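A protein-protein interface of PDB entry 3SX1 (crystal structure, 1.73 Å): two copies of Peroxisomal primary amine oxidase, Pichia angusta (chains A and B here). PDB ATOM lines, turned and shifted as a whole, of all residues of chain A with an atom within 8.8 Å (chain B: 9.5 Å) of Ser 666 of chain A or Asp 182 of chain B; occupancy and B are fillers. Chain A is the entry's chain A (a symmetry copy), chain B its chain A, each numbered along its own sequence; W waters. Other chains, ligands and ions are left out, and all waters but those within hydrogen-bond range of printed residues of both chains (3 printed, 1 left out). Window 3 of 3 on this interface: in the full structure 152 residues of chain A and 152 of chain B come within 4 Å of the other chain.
NH2 of Arg 178 of chain B is in salt-bridge range of OD2 of Asp 378 of chain A.
The side-chain amino group of Lys 669 of chain A lies within salt-bridge range of the side-chain carboxylate of Glu 181 of chain B (3.8 Å).
N of Thr 665 of chain A is in hydrogen-bond range of OD1 of Asp 182 of chain B, 3.2 Å away.
OD2 of Asp 182 of chain B lies within hydrogen-bond range of OG of Ser 666 of chain A (2.6 Å).
OH of Tyr 224 of chain B is in hydrogen-bond range of O of Met 663 of chain A, 2.8 Å away.
No position is printed for both chains.
OE1 of Gln 185 of chain B sits at hydrogen-bond distance from NH2 of Arg 178 of chain B, at 2.9 Å.
The side-chain amino group (NZ) of Lys 226 of chain B is in salt-bridge range of the side-chain carboxylate (OD2) of Asp 182 of chain B.
OD2 of Asp 381 of chain A is in hydrogen-bond range of OG1 of Thr 385 of chain A, 2.7 Å away.
OG1 of Thr 385 of chain A lies within hydrogen-bond range of OG1 of Thr 665 of chain A.
OG1 of Thr 664 of chain A sits at hydrogen-bond distance from OG of Ser 666 of chain A, at 3.3 Å.
N of Thr 664 of chain A sits at hydrogen-bond distance from OE1 of Glu 667 of chain A (2.9 Å).
Among the printed residues, pairs that only touch across the chains: Thr 385 of chain A with Tyr 224 of chain B, Thr 664 of chain A with Asp 182 of chain B, Thr 664 of chain A with Tyr 224 of chain B, Thr 665 of chain A with Glu 181 of chain B and Ser 666 of chain A with Glu 181 of chain B.
Printed residues of chain A that touch a printed residue of chain B: Asp 378, Thr 385, Met 663, Thr 664, Thr 665, Ser 666 and Lys 669.
Hydrophobic or aromatic side chains of chain B that line the printed part of chain A: Tyr 224.
Among the printed residues, Asp or Glu carboxylates within 4 Å of a Lys or Arg side-chain nitrogen of the other chain: Asp 378 of chain A with Arg 178 of chain B (3.0 Å) and Lys 669 of chain A with Glu 181 of chain B (3.8 Å).
Water W3 lies within hydrogen-bond range of the side-chain carboxylate (OD2) of Asp 378 of chain A (2.6 Å), the side-chain hydroxyl (OG1) of Thr 665 of chain A (2.8 Å) and the guanidinium group (NH1) of Arg 178 of chain B (2.9 Å).
Water W2 lies within hydrogen-bond range of OG1 of Thr 664 of chain A (3.0 Å), NZ of Lys 226 of chain B (3.1 Å) and OE2 of Glu 667 of chain A (3.2 Å).
Water W1 lies within hydrogen-bond range of N of Thr 665 of chain A (3.0 Å) and O of Asp 182 of chain B (3.3 Å).
Ala 384 of chain A touches none of the printed residues of chain B.
Thr 664 of chain A touches two residues of chain B.
Thr 665 of chain A touches just these residues of chain B: Glu 181 and Asp 182.
Ser 666 of chain A touches two residues of chain B.
No residue of chain B comes within 4 Å of Ala 668 of chain A.
Of the printed residues of chain A, Arg 178 of chain B touches Asp 378.
Asp 182 of chain B touches three residues of chain A.
Of the printed residues of chain A, Tyr 224 of chain B touches Thr 385 (3.5 Å), Met 663 (2.8 Å) and Thr 664 (3.5 Å).
His 227 of chain B touches none of the printed residues of chain A.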
ATOM      1  N   ASP A 378      26.954  -6.633 -11.018  1.00  0.00           N
ATOM      2  CA  ASP A 378      27.524  -6.225 -12.325  1.00  0.00           C
ATOM      3  C   ASP A 378      29.022  -5.922 -12.148  1.00  0.00           C
ATOM      4  O   ASP A 378      29.386  -5.010 -11.388  1.00  0.00           O
ATOM      5  CB  ASP A 378      26.795  -4.950 -12.821  1.00  0.00           C
ATOM      6  CG  ASP A 378      27.009  -4.673 -14.336  1.00  0.00           C
ATOM      7  OD1 ASP A 378      28.048  -5.048 -14.872  1.00  0.00           O
ATOM      8  OD2 ASP A 378      26.134  -4.066 -14.988  1.00  0.00           O
ATOM      9  N   ASP A 381      30.746  -1.932 -12.562  1.00  0.00           N
ATOM     10  CA  ASP A 381      31.059  -0.967 -11.499  1.00  0.00           C
ATOM     11  C   ASP A 381      31.640  -1.629 -10.253  1.00  0.00           C
ATOM     12  O   ASP A 381      31.383  -1.220  -9.112  1.00  0.00           O
ATOM     13  CB  ASP A 381      29.880  -0.055 -11.185  1.00  0.00           C
ATOM     14  CG  ASP A 381      28.580  -0.827 -10.848  1.00  0.00           C
ATOM     15  OD1 ASP A 381      28.656  -2.045 -10.532  1.00  0.00           O
ATOM     16  OD2 ASP A 381      27.507  -0.162 -10.786  1.00  0.00           O
ATOM     17  N   ALA A 384      29.172  -2.825  -7.523  1.00  0.00           N
ATOM     18  CA  ALA A 384      28.305  -1.888  -6.816  1.00  0.00           C
ATOM     19  C   ALA A 384      26.851  -2.136  -7.192  1.00  0.00           C
ATOM     20  O   ALA A 384      25.954  -1.993  -6.355  1.00  0.00           O
ATOM     21  CB  ALA A 384      28.683  -0.426  -7.160  1.00  0.00           C
ATOM     22  N   THR A 385      26.602  -2.386  -8.469  1.00  0.00           N
ATOM     23  CA  THR A 385      25.267  -2.828  -8.901  1.00  0.00           C
ATOM     24  C   THR A 385      25.057  -4.269  -8.467  1.00  0.00           C
ATOM     25  O   THR A 385      25.841  -5.151  -8.859  1.00  0.00           O
ATOM     26  CB  THR A 385      25.133  -2.754 -10.439  1.00  0.00           C
ATOM     27  OG1 THR A 385      25.124  -1.381 -10.830  1.00  0.00           O
ATOM     28  CG2 THR A 385      23.812  -3.361 -10.939  1.00  0.00           C
ATOM     29  N   MET A 663      21.157  -2.542  -4.929  1.00  0.00           N
ATOM     30  CA  MET A 663      21.572  -1.240  -5.454  1.00  0.00           C
ATOM     31  C   MET A 663      21.596  -1.346  -6.971  1.00  0.00           C
ATOM     32  O   MET A 663      22.214  -2.259  -7.525  1.00  0.00           O
ATOM     33  CB  MET A 663      22.957  -0.876  -4.926  1.00  0.00           C
ATOM     34  CG  MET A 663      23.519   0.420  -5.517  1.00  0.00           C
ATOM     35  SD  MET A 663      25.014   1.014  -4.685  1.00  0.00           S
ATOM     36  CE  MET A 663      24.336   1.695  -3.164  1.00  0.00           C
ATOM     37  N   THR A 664      20.904  -0.421  -7.634  1.00  0.00           N
ATOM     38  CA  THR A 664      20.875  -0.382  -9.093  1.00  0.00           C
ATOM     39  C   THR A 664      22.084   0.412  -9.601  1.00  0.00           C
ATOM     40  O   THR A 664      22.803   1.047  -8.841  1.00  0.00           O
ATOM     41  CB  THR A 664      19.628   0.339  -9.608  1.00  0.00           C
ATOM     42  OG1 THR A 664      19.696   1.708  -9.156  1.00  0.00           O
ATOM     43  CG2 THR A 664      18.337  -0.300  -9.071  1.00  0.00           C
ATOM     44  N   THR A 665      22.311   0.353 -10.902  1.00  0.00           N
ATOM     45  CA  THR A 665      23.421   1.058 -11.514  1.00  0.00           C
ATOM     46  C   THR A 665      23.306   2.578 -11.342  1.00  0.00           C
ATOM     47  O   THR A 665      24.288   3.251 -11.025  1.00  0.00           O
ATOM     48  CB  THR A 665      23.483   0.674 -12.984  1.00  0.00           C
ATOM     49  OG1 THR A 665      23.919  -0.690 -13.038  1.00  0.00           O
ATOM     50  CG2 THR A 665      24.478   1.549 -13.758  1.00  0.00           C
ATOM     51  N   SER A 666      22.113   3.106 -11.539  1.00  0.00           N
ATOM     52  CA  SER A 666      21.874   4.550 -11.344  1.00  0.00           C
ATOM     53  C   SER A 666      22.078   4.965  -9.890  1.00  0.00           C
ATOM     54  O   SER A 666      22.693   6.011  -9.616  1.00  0.00           O
ATOM     55  CB  SER A 666      20.475   4.944 -11.826  1.00  0.00           C
ATOM     56  OG  SER A 666      19.422   4.322 -11.074  1.00  0.00           O
ATOM     57  N   GLU A 667      21.595   4.142  -8.958  1.00  0.00           N
ATOM     58  CA  GLU A 667      21.836   4.416  -7.546  1.00  0.00           C
ATOM     59  C   GLU A 667      23.328   4.407  -7.235  1.00  0.00           C
ATOM     60  O   GLU A 667      23.818   5.292  -6.512  1.00  0.00           O
ATOM     61  CB  GLU A 667      21.094   3.433  -6.649  1.00  0.00           C
ATOM     62  CG  GLU A 667      19.618   3.601  -6.689  1.00  0.00           C
ATOM     63  CD  GLU A 667      18.867   2.466  -6.010  1.00  0.00           C
ATOM     64  OE1 GLU A 667      19.443   1.359  -5.847  1.00  0.00           O
ATOM     65  OE2 GLU A 667      17.659   2.652  -5.731  1.00  0.00           O
ATOM     66  N   ALA A 668      24.060   3.419  -7.762  1.00  0.00           N
ATOM     67  CA  ALA A 668      25.498   3.354  -7.494  1.00  0.00           C
ATOM     68  C   ALA A 668      26.227   4.595  -8.029  1.00  0.00           C
ATOM     69  O   ALA A 668      27.189   5.078  -7.403  1.00  0.00           O
ATOM     70  CB  ALA A 668      26.116   2.089  -8.083  1.00  0.00           C
ATOM     71  N   LYS A 669      25.796   5.065  -9.199  1.00  0.00           N
ATOM     72  CA  LYS A 669      26.365   6.284  -9.809  1.00  0.00           C
ATOM     73  C   LYS A 669      26.129   7.513  -8.945  1.00  0.00           C
ATOM     74  O   LYS A 669      26.979   8.415  -8.889  1.00  0.00           O
ATOM     75  CB  LYS A 669      25.805   6.519 -11.214  1.00  0.00           C
ATOM     76  CG  LYS A 669      26.549   5.785 -12.309  1.00  0.00           C
ATOM     77  CD  LYS A 669      26.003   6.220 -13.672  1.00  0.00           C
ATOM     78  CE  LYS A 669      26.036   5.085 -14.670  1.00  0.00           C
ATOM     79  NZ  LYS A 669      27.253   5.101 -15.528  1.00  0.00           N
ATOM     80  N   ARG A 670      24.974   7.574  -8.295  1.00  0.00           N
ATOM     81  CA  ARG A 670      24.647   8.724  -7.459  1.00  0.00           C
ATOM     82  C   ARG A 670      25.432   8.696  -6.152  1.00  0.00           C
ATOM     83  O   ARG A 670      25.834   9.738  -5.643  1.00  0.00           O
ATOM     84  CB  ARG A 670      23.145   8.785  -7.182  1.00  0.00           C
ATOM     85  CG  ARG A 670      22.348   9.348  -8.330  1.00  0.00           C
ATOM     86  CD  ARG A 670      21.035   9.909  -7.845  1.00  0.00           C
ATOM     87  NE  ARG A 670      20.270   8.900  -7.118  1.00  0.00           N
ATOM     88  CZ  ARG A 670      19.515   7.976  -7.705  1.00  0.00           C
ATOM     89  NH1 ARG A 670      19.414   7.948  -9.028  1.00  0.00           N
ATOM     90  NH2 ARG A 670      18.859   7.083  -6.968  1.00  0.00           N
ATOM     91  N   ALA A 671      25.697   7.495  -5.650  1.00  0.00           N
ATOM     92  CA  ALA A 671      26.480   7.302  -4.434  1.00  0.00           C
ATOM     93  C   ALA A 671      27.975   7.628  -4.574  1.00  0.00           C
ATOM     94  O   ALA A 671      28.669   7.746  -3.568  1.00  0.00           O
ATOM     95  CB  ALA A 671      26.287   5.879  -3.894  1.00  0.00           C
ATOM     96  N   VAL A 672      28.482   7.757  -5.797  1.00  0.00           N
ATOM     97  CA  VAL A 672      29.786   8.404  -5.996  1.00  0.00           C
ATOM     98  C   VAL A 672      29.692   9.840  -6.553  1.00  0.00           C
ATOM     99  O   VAL A 672      29.460  10.077  -7.747  1.00  0.00           O
ATOM    100  CB  VAL A 672      30.782   7.539  -6.817  1.00  0.00           C
ATOM    101  CG1 VAL A 672      30.049   6.584  -7.749  1.00  0.00           C
ATOM    102  CG2 VAL A 672      31.761   8.427  -7.596  1.00  0.00           C
ATOM    103  N   HIS B 149      25.728   3.956 -26.528  1.00  0.00           N
ATOM    104  CA  HIS B 149      25.879   3.880 -25.069  1.00  0.00           C
ATOM    105  C   HIS B 149      24.915   2.861 -24.456  1.00  0.00           C
ATOM    106  O   HIS B 149      25.059   2.485 -23.277  1.00  0.00           O
ATOM    107  CB  HIS B 149      25.697   5.249 -24.400  1.00  0.00           C
ATOM    108  CG  HIS B 149      24.288   5.754 -24.437  1.00  0.00           C
ATOM    109  ND1 HIS B 149      23.743   6.367 -25.551  1.00  0.00           N
ATOM    110  CD2 HIS B 149      23.302   5.712 -23.509  1.00  0.00           C
ATOM    111  CE1 HIS B 149      22.485   6.688 -25.304  1.00  0.00           C
ATOM    112  NE2 HIS B 149      22.195   6.309 -24.070  1.00  0.00           N
ATOM    113  N   TYR B 152      26.027  -3.086 -24.779  1.00  0.00           N
ATOM    114  CA  TYR B 152      26.903  -3.608 -23.747  1.00  0.00           C
ATOM    115  C   TYR B 152      27.450  -4.923 -24.277  1.00  0.00           C
ATOM    116  O   TYR B 152      26.889  -5.553 -25.200  1.00  0.00           O
ATOM    117  CB  TYR B 152      26.070  -3.899 -22.486  1.00  0.00           C
ATOM    118  CG  TYR B 152      25.648  -2.623 -21.773  1.00  0.00           C
ATOM    119  CD1 TYR B 152      24.561  -1.860 -22.218  1.00  0.00           C
ATOM    120  CD2 TYR B 152      26.308  -2.222 -20.609  1.00  0.00           C
ATOM    121  CE1 TYR B 152      24.249  -0.637 -21.591  1.00  0.00           C
ATOM    122  CE2 TYR B 152      25.952  -1.048 -19.939  1.00  0.00           C
ATOM    123  CZ  TYR B 152      24.915  -0.274 -20.438  1.00  0.00           C
ATOM    124  OH  TYR B 152      24.556   0.861 -19.712  1.00  0.00           O
ATOM    125  N   TYR B 177      21.791  -5.371 -25.286  1.00  0.00           N
ATOM    126  CA  TYR B 177      21.285  -3.995 -25.406  1.00  0.00           C
ATOM    127  C   TYR B 177      20.496  -3.692 -24.117  1.00  0.00           C
ATOM    128  O   TYR B 177      19.739  -4.549 -23.632  1.00  0.00           O
ATOM    129  CB  TYR B 177      20.316  -3.969 -26.601  1.00  0.00           C
ATOM    130  CG  TYR B 177      19.473  -2.712 -26.682  1.00  0.00           C
ATOM    131  CD1 TYR B 177      20.035  -1.509 -27.133  1.00  0.00           C
ATOM    132  CD2 TYR B 177      18.120  -2.731 -26.321  1.00  0.00           C
ATOM    133  CE1 TYR B 177      19.275  -0.351 -27.224  1.00  0.00           C
ATOM    134  CE2 TYR B 177      17.339  -1.568 -26.422  1.00  0.00           C
ATOM    135  CZ  TYR B 177      17.939  -0.387 -26.862  1.00  0.00           C
ATOM    136  OH  TYR B 177      17.188   0.789 -26.921  1.00  0.00           O
ATOM    137  N   ARG B 178      20.635  -2.468 -23.583  1.00  0.00           N
ATOM    138  CA  ARG B 178      19.825  -2.016 -22.439  1.00  0.00           C
ATOM    139  C   ARG B 178      19.033  -0.784 -22.871  1.00  0.00           C
ATOM    140  O   ARG B 178      19.639   0.188 -23.361  1.00  0.00           O
ATOM    141  CB  ARG B 178      20.716  -1.590 -21.260  1.00  0.00           C
ATOM    142  CG  ARG B 178      21.520  -2.755 -20.650  1.00  0.00           C
ATOM    143  CD  ARG B 178      22.143  -2.359 -19.308  1.00  0.00           C
ATOM    144  NE  ARG B 178      23.234  -3.271 -18.976  1.00  0.00           N
ATOM    145  CZ  ARG B 178      24.050  -3.094 -17.953  1.00  0.00           C
ATOM    146  NH1 ARG B 178      23.872  -2.044 -17.139  1.00  0.00           N
ATOM    147  NH2 ARG B 178      25.101  -3.889 -17.801  1.00  0.00           N
ATOM    148  N   SER B 179      17.722  -0.785 -22.618  1.00  0.00           N
ATOM    149  CA  SER B 179      16.926   0.421 -22.889  1.00  0.00           C
ATOM    150  C   SER B 179      17.193   1.492 -21.833  1.00  0.00           C
ATOM    151  O   SER B 179      17.139   2.701 -22.134  1.00  0.00           O
ATOM    152  CB  SER B 179      15.434   0.096 -22.990  1.00  0.00           C
ATOM    153  OG  SER B 179      14.904  -0.281 -21.739  1.00  0.00           O
ATOM    154  N   ASP B 180      17.545   1.050 -20.626  1.00  0.00           N
ATOM    155  CA  ASP B 180      17.866   1.935 -19.522  1.00  0.00           C
ATOM    156  C   ASP B 180      19.014   1.294 -18.767  1.00  0.00           C
ATOM    157  O   ASP B 180      19.099   0.037 -18.716  1.00  0.00           O
ATOM    158  CB  ASP B 180      16.635   2.029 -18.598  1.00  0.00           C
ATOM    159  CG  ASP B 180      16.920   2.826 -17.323  1.00  0.00           C
ATOM    160  OD1 ASP B 180      16.899   4.070 -17.374  1.00  0.00           O
ATOM    161  OD2 ASP B 180      17.196   2.217 -16.275  1.00  0.00           O
ATOM    162  N   GLU B 181      19.940   2.113 -18.259  1.00  0.00           N
ATOM    163  CA  GLU B 181      21.123   1.553 -17.610  1.00  0.00           C
ATOM    164  C   GLU B 181      20.785   0.524 -16.480  1.00  0.00           C
ATOM    165  O   GLU B 181      21.636  -0.296 -16.128  1.00  0.00           O
ATOM    166  CB  GLU B 181      22.032   2.676 -17.090  1.00  0.00           C
ATOM    167  CG  GLU B 181      21.463   3.412 -15.893  1.00  0.00           C
ATOM    168  CD  GLU B 181      22.279   4.679 -15.510  1.00  0.00           C
ATOM    169  OE1 GLU B 181      23.455   4.793 -15.901  1.00  0.00           O
ATOM    170  OE2 GLU B 181      21.741   5.533 -14.782  1.00  0.00           O
ATOM    171  N   ASP B 182      19.604   0.621 -15.858  1.00  0.00           N
ATOM    172  CA  ASP B 182      19.280  -0.260 -14.724  1.00  0.00           C
ATOM    173  C   ASP B 182      18.650  -1.568 -15.180  1.00  0.00           C
ATOM    174  O   ASP B 182      18.338  -2.457 -14.355  1.00  0.00           O
ATOM    175  CB  ASP B 182      18.336   0.445 -13.723  1.00  0.00           C
ATOM    176  CG  ASP B 182      19.016   1.593 -12.984  1.00  0.00           C
ATOM    177  OD1 ASP B 182      20.248   1.635 -12.947  1.00  0.00           O
ATOM    178  OD2 ASP B 182      18.288   2.399 -12.336  1.00  0.00           O
ATOM    179  N   ASP B 183      18.489  -1.725 -16.497  1.00  0.00           N
ATOM    180  CA  ASP B 183      17.927  -2.992 -17.018  1.00  0.00           C
ATOM    181  C   ASP B 183      18.889  -4.115 -16.778  1.00  0.00           C
ATOM    182  O   ASP B 183      20.107  -3.909 -16.754  1.00  0.00           O
ATOM    183  CB  ASP B 183      17.720  -2.948 -18.536  1.00  0.00           C
ATOM    184  CG  ASP B 183      16.563  -2.080 -18.957  1.00  0.00           C
ATOM    185  OD1 ASP B 183      15.601  -1.851 -18.187  1.00  0.00           O
ATOM    186  OD2 ASP B 183      16.572  -1.702 -20.136  1.00  0.00           O
ATOM    187  N   SER B 184      18.344  -5.324 -16.736  1.00  0.00           N
ATOM    188  CA  SER B 184      19.153  -6.517 -16.952  1.00  0.00           C
ATOM    189  C   SER B 184      19.187  -6.792 -18.440  1.00  0.00           C
ATOM    190  O   SER B 184      18.170  -7.030 -19.066  1.00  0.00           O
ATOM    191  CB  SER B 184      18.548  -7.712 -16.229  1.00  0.00           C
ATOM    192  OG  SER B 184      19.482  -8.797 -16.274  1.00  0.00           O
ATOM    193  N   GLN B 185      20.380  -6.749 -19.005  1.00  0.00           N
ATOM    194  CA  GLN B 185      20.525  -6.716 -20.456  1.00  0.00           C
ATOM    195  C   GLN B 185      20.232  -8.083 -21.101  1.00  0.00           C
ATOM    196  O   GLN B 185      20.057  -8.173 -22.328  1.00  0.00           O
ATOM    197  CB  GLN B 185      21.972  -6.297 -20.784  1.00  0.00           C
ATOM    198  CG  GLN B 185      23.029  -7.411 -20.395  1.00  0.00           C
ATOM    199  CD  GLN B 185      24.436  -6.841 -20.299  1.00  0.00           C
ATOM    200  OE1 GLN B 185      24.595  -5.648 -20.079  1.00  0.00           O
ATOM    201  NE2 GLN B 185      25.448  -7.676 -20.530  1.00  0.00           N
ATOM    202  N   TYR B 186      20.116  -9.152 -20.288  1.00  0.00           N
ATOM    203  CA  TYR B 186      20.158 -10.497 -20.891  1.00  0.00           C
ATOM    204  C   TYR B 186      18.869 -10.916 -21.590  1.00  0.00           C
ATOM    205  O   TYR B 186      18.870 -11.895 -22.313  1.00  0.00           O
ATOM    206  CB  TYR B 186      20.566 -11.558 -19.839  1.00  0.00           C
ATOM    207  CG  TYR B 186      21.965 -11.261 -19.331  1.00  0.00           C
ATOM    208  CD1 TYR B 186      23.082 -11.718 -20.061  1.00  0.00           C
ATOM    209  CD2 TYR B 186      22.179 -10.484 -18.193  1.00  0.00           C
ATOM    210  CE1 TYR B 186      24.390 -11.427 -19.648  1.00  0.00           C
ATOM    211  CE2 TYR B 186      23.481 -10.200 -17.763  1.00  0.00           C
ATOM    212  CZ  TYR B 186      24.567 -10.676 -18.494  1.00  0.00           C
ATOM    213  OH  TYR B 186      25.852 -10.448 -18.063  1.00  0.00           O
ATOM    214  N   HIS B 220      12.329  -5.194 -21.286  1.00  0.00           N
ATOM    215  CA  HIS B 220      13.385  -5.984 -20.637  1.00  0.00           C
ATOM    216  C   HIS B 220      12.814  -6.796 -19.507  1.00  0.00           C
ATOM    217  O   HIS B 220      11.818  -6.383 -18.882  1.00  0.00           O
ATOM    218  CB  HIS B 220      14.472  -5.073 -20.107  1.00  0.00           C
ATOM    219  CG  HIS B 220      15.455  -4.662 -21.157  1.00  0.00           C
ATOM    220  ND1 HIS B 220      15.107  -3.850 -22.222  1.00  0.00           N
ATOM    221  CD2 HIS B 220      16.713  -5.102 -21.411  1.00  0.00           C
ATOM    222  CE1 HIS B 220      16.142  -3.740 -23.038  1.00  0.00           C
ATOM    223  NE2 HIS B 220      17.145  -4.449 -22.539  1.00  0.00           N
ATOM    224  N   ALA B 221      13.392  -7.988 -19.306  1.00  0.00           N
ATOM    225  CA  ALA B 221      12.994  -8.871 -18.192  1.00  0.00           C
ATOM    226  C   ALA B 221      13.792  -8.491 -16.937  1.00  0.00           C
ATOM    227  O   ALA B 221      14.925  -8.939 -16.736  1.00  0.00           O
ATOM    228  CB  ALA B 221      13.284 -10.302 -18.593  1.00  0.00           C
ATOM    229  N   ASN B 222      13.206  -7.629 -16.101  1.00  0.00           N
ATOM    230  CA  ASN B 222      13.946  -7.003 -15.010  1.00  0.00           C
ATOM    231  C   ASN B 222      13.570  -7.591 -13.645  1.00  0.00           C
ATOM    232  O   ASN B 222      12.561  -8.293 -13.529  1.00  0.00           O
ATOM    233  CB  ASN B 222      13.717  -5.504 -15.025  1.00  0.00           C
ATOM    234  CG  ASN B 222      14.495  -4.835 -16.129  1.00  0.00           C
ATOM    235  OD1 ASN B 222      15.590  -5.268 -16.450  1.00  0.00           O
ATOM    236  ND2 ASN B 222      13.933  -3.777 -16.723  1.00  0.00           N
ATOM    237  N   PHE B 223      14.383  -7.319 -12.622  1.00  0.00           N
ATOM    238  CA  PHE B 223      14.212  -7.989 -11.338  1.00  0.00           C
ATOM    239  C   PHE B 223      14.445  -7.172 -10.074  1.00  0.00           C
ATOM    240  O   PHE B 223      14.325  -7.703  -8.973  1.00  0.00           O
ATOM    241  CB  PHE B 223      15.052  -9.272 -11.276  1.00  0.00           C
ATOM    242  CG  PHE B 223      16.537  -9.048 -11.540  1.00  0.00           C
ATOM    243  CD1 PHE B 223      17.348  -8.434 -10.606  1.00  0.00           C
ATOM    244  CD2 PHE B 223      17.112  -9.500 -12.740  1.00  0.00           C
ATOM    245  CE1 PHE B 223      18.726  -8.243 -10.883  1.00  0.00           C
ATOM    246  CE2 PHE B 223      18.448  -9.307 -13.005  1.00  0.00           C
ATOM    247  CZ  PHE B 223      19.255  -8.691 -12.075  1.00  0.00           C
ATOM    248  N   TYR B 224      14.720  -5.868 -10.189  1.00  0.00           N
ATOM    249  CA  TYR B 224      14.809  -5.069  -8.953  1.00  0.00           C
ATOM    250  C   TYR B 224      13.406  -4.740  -8.441  1.00  0.00           C
ATOM    251  O   TYR B 224      12.425  -4.827  -9.169  1.00  0.00           O
ATOM    252  CB  TYR B 224      15.594  -3.757  -9.202  1.00  0.00           C
ATOM    253  CG  TYR B 224      17.098  -3.946  -9.141  1.00  0.00           C
ATOM    254  CD1 TYR B 224      17.802  -4.516 -10.208  1.00  0.00           C
ATOM    255  CD2 TYR B 224      17.808  -3.576  -8.007  1.00  0.00           C
ATOM    256  CE1 TYR B 224      19.180  -4.705 -10.137  1.00  0.00           C
ATOM    257  CE2 TYR B 224      19.131  -3.823  -7.892  1.00  0.00           C
ATOM    258  CZ  TYR B 224      19.853  -4.325  -8.996  1.00  0.00           C
ATOM    259  OH  TYR B 224      21.231  -4.446  -8.908  1.00  0.00           O
ATOM    260  N   PRO B 225      13.301  -4.372  -7.158  1.00  0.00           N
ATOM    261  CA  PRO B 225      11.979  -4.076  -6.625  1.00  0.00           C
ATOM    262  C   PRO B 225      11.173  -3.070  -7.455  1.00  0.00           C
ATOM    263  O   PRO B 225       9.988  -3.274  -7.659  1.00  0.00           O
ATOM    264  CB  PRO B 225      12.296  -3.543  -5.224  1.00  0.00           C
ATOM    265  CG  PRO B 225      13.445  -4.442  -4.788  1.00  0.00           C
ATOM    266  CD  PRO B 225      14.310  -4.510  -6.090  1.00  0.00           C
ATOM    267  N   LYS B 226      11.797  -2.010  -7.964  1.00  0.00           N
ATOM    268  CA  LYS B 226      11.000  -1.037  -8.715  1.00  0.00           C
ATOM    269  C   LYS B 226      10.391  -1.672  -9.942  1.00  0.00           C
ATOM    270  O   LYS B 226       9.265  -1.335 -10.333  1.00  0.00           O
ATOM    271  CB  LYS B 226      11.813   0.233  -9.081  1.00  0.00           C
ATOM    272  CG  LYS B 226      13.062  -0.026  -9.933  1.00  0.00           C
ATOM    273  CD  LYS B 226      13.776   1.298 -10.260  1.00  0.00           C
ATOM    274  CE  LYS B 226      14.804   1.097 -11.382  1.00  0.00           C
ATOM    275  NZ  LYS B 226      15.569   2.376 -11.571  1.00  0.00           N
ATOM    276  N   HIS B 227      11.123  -2.622 -10.544  1.00  0.00           N
ATOM    277  CA  HIS B 227      10.615  -3.332 -11.717  1.00  0.00           C
ATOM    278  C   HIS B 227       9.501  -4.316 -11.346  1.00  0.00           C
ATOM    279  O   HIS B 227       8.543  -4.483 -12.102  1.00  0.00           O
ATOM    280  CB  HIS B 227      11.743  -4.108 -12.423  1.00  0.00           C
ATOM    281  CG  HIS B 227      12.946  -3.275 -12.759  1.00  0.00           C
ATOM    282  ND1 HIS B 227      14.209  -3.584 -12.298  1.00  0.00           N
ATOM    283  CD2 HIS B 227      13.109  -2.257 -13.643  1.00  0.00           C
ATOM    284  CE1 HIS B 227      15.093  -2.754 -12.833  1.00  0.00           C
ATOM    285  NE2 HIS B 227      14.450  -1.930 -13.645  1.00  0.00           N
ATOM    286  N   ILE B 428      22.763 -15.127 -13.698  1.00  0.00           N
ATOM    287  CA  ILE B 428      21.911 -15.023 -14.868  1.00  0.00           C
ATOM    288  C   ILE B 428      22.319 -16.005 -15.961  1.00  0.00           C
ATOM    289  O   ILE B 428      23.501 -16.171 -16.242  1.00  0.00           O
ATOM    290  CB  ILE B 428      21.960 -13.579 -15.389  1.00  0.00           C
ATOM    291  CG1 ILE B 428      21.434 -12.673 -14.265  1.00  0.00           C
ATOM    292  CG2 ILE B 428      21.065 -13.425 -16.616  1.00  0.00           C
ATOM    293  CD1 ILE B 428      21.442 -11.245 -14.591  1.00  0.00           C
HETATM  294  O   HOH W   1      20.709  -1.884 -12.061  1.00  0.00           O
HETATM  295  O   HOH W   2      16.991   2.910  -8.891  1.00  0.00           O
HETATM  296  O   HOH W   3      25.745  -1.504 -14.981  1.00  0.00           O
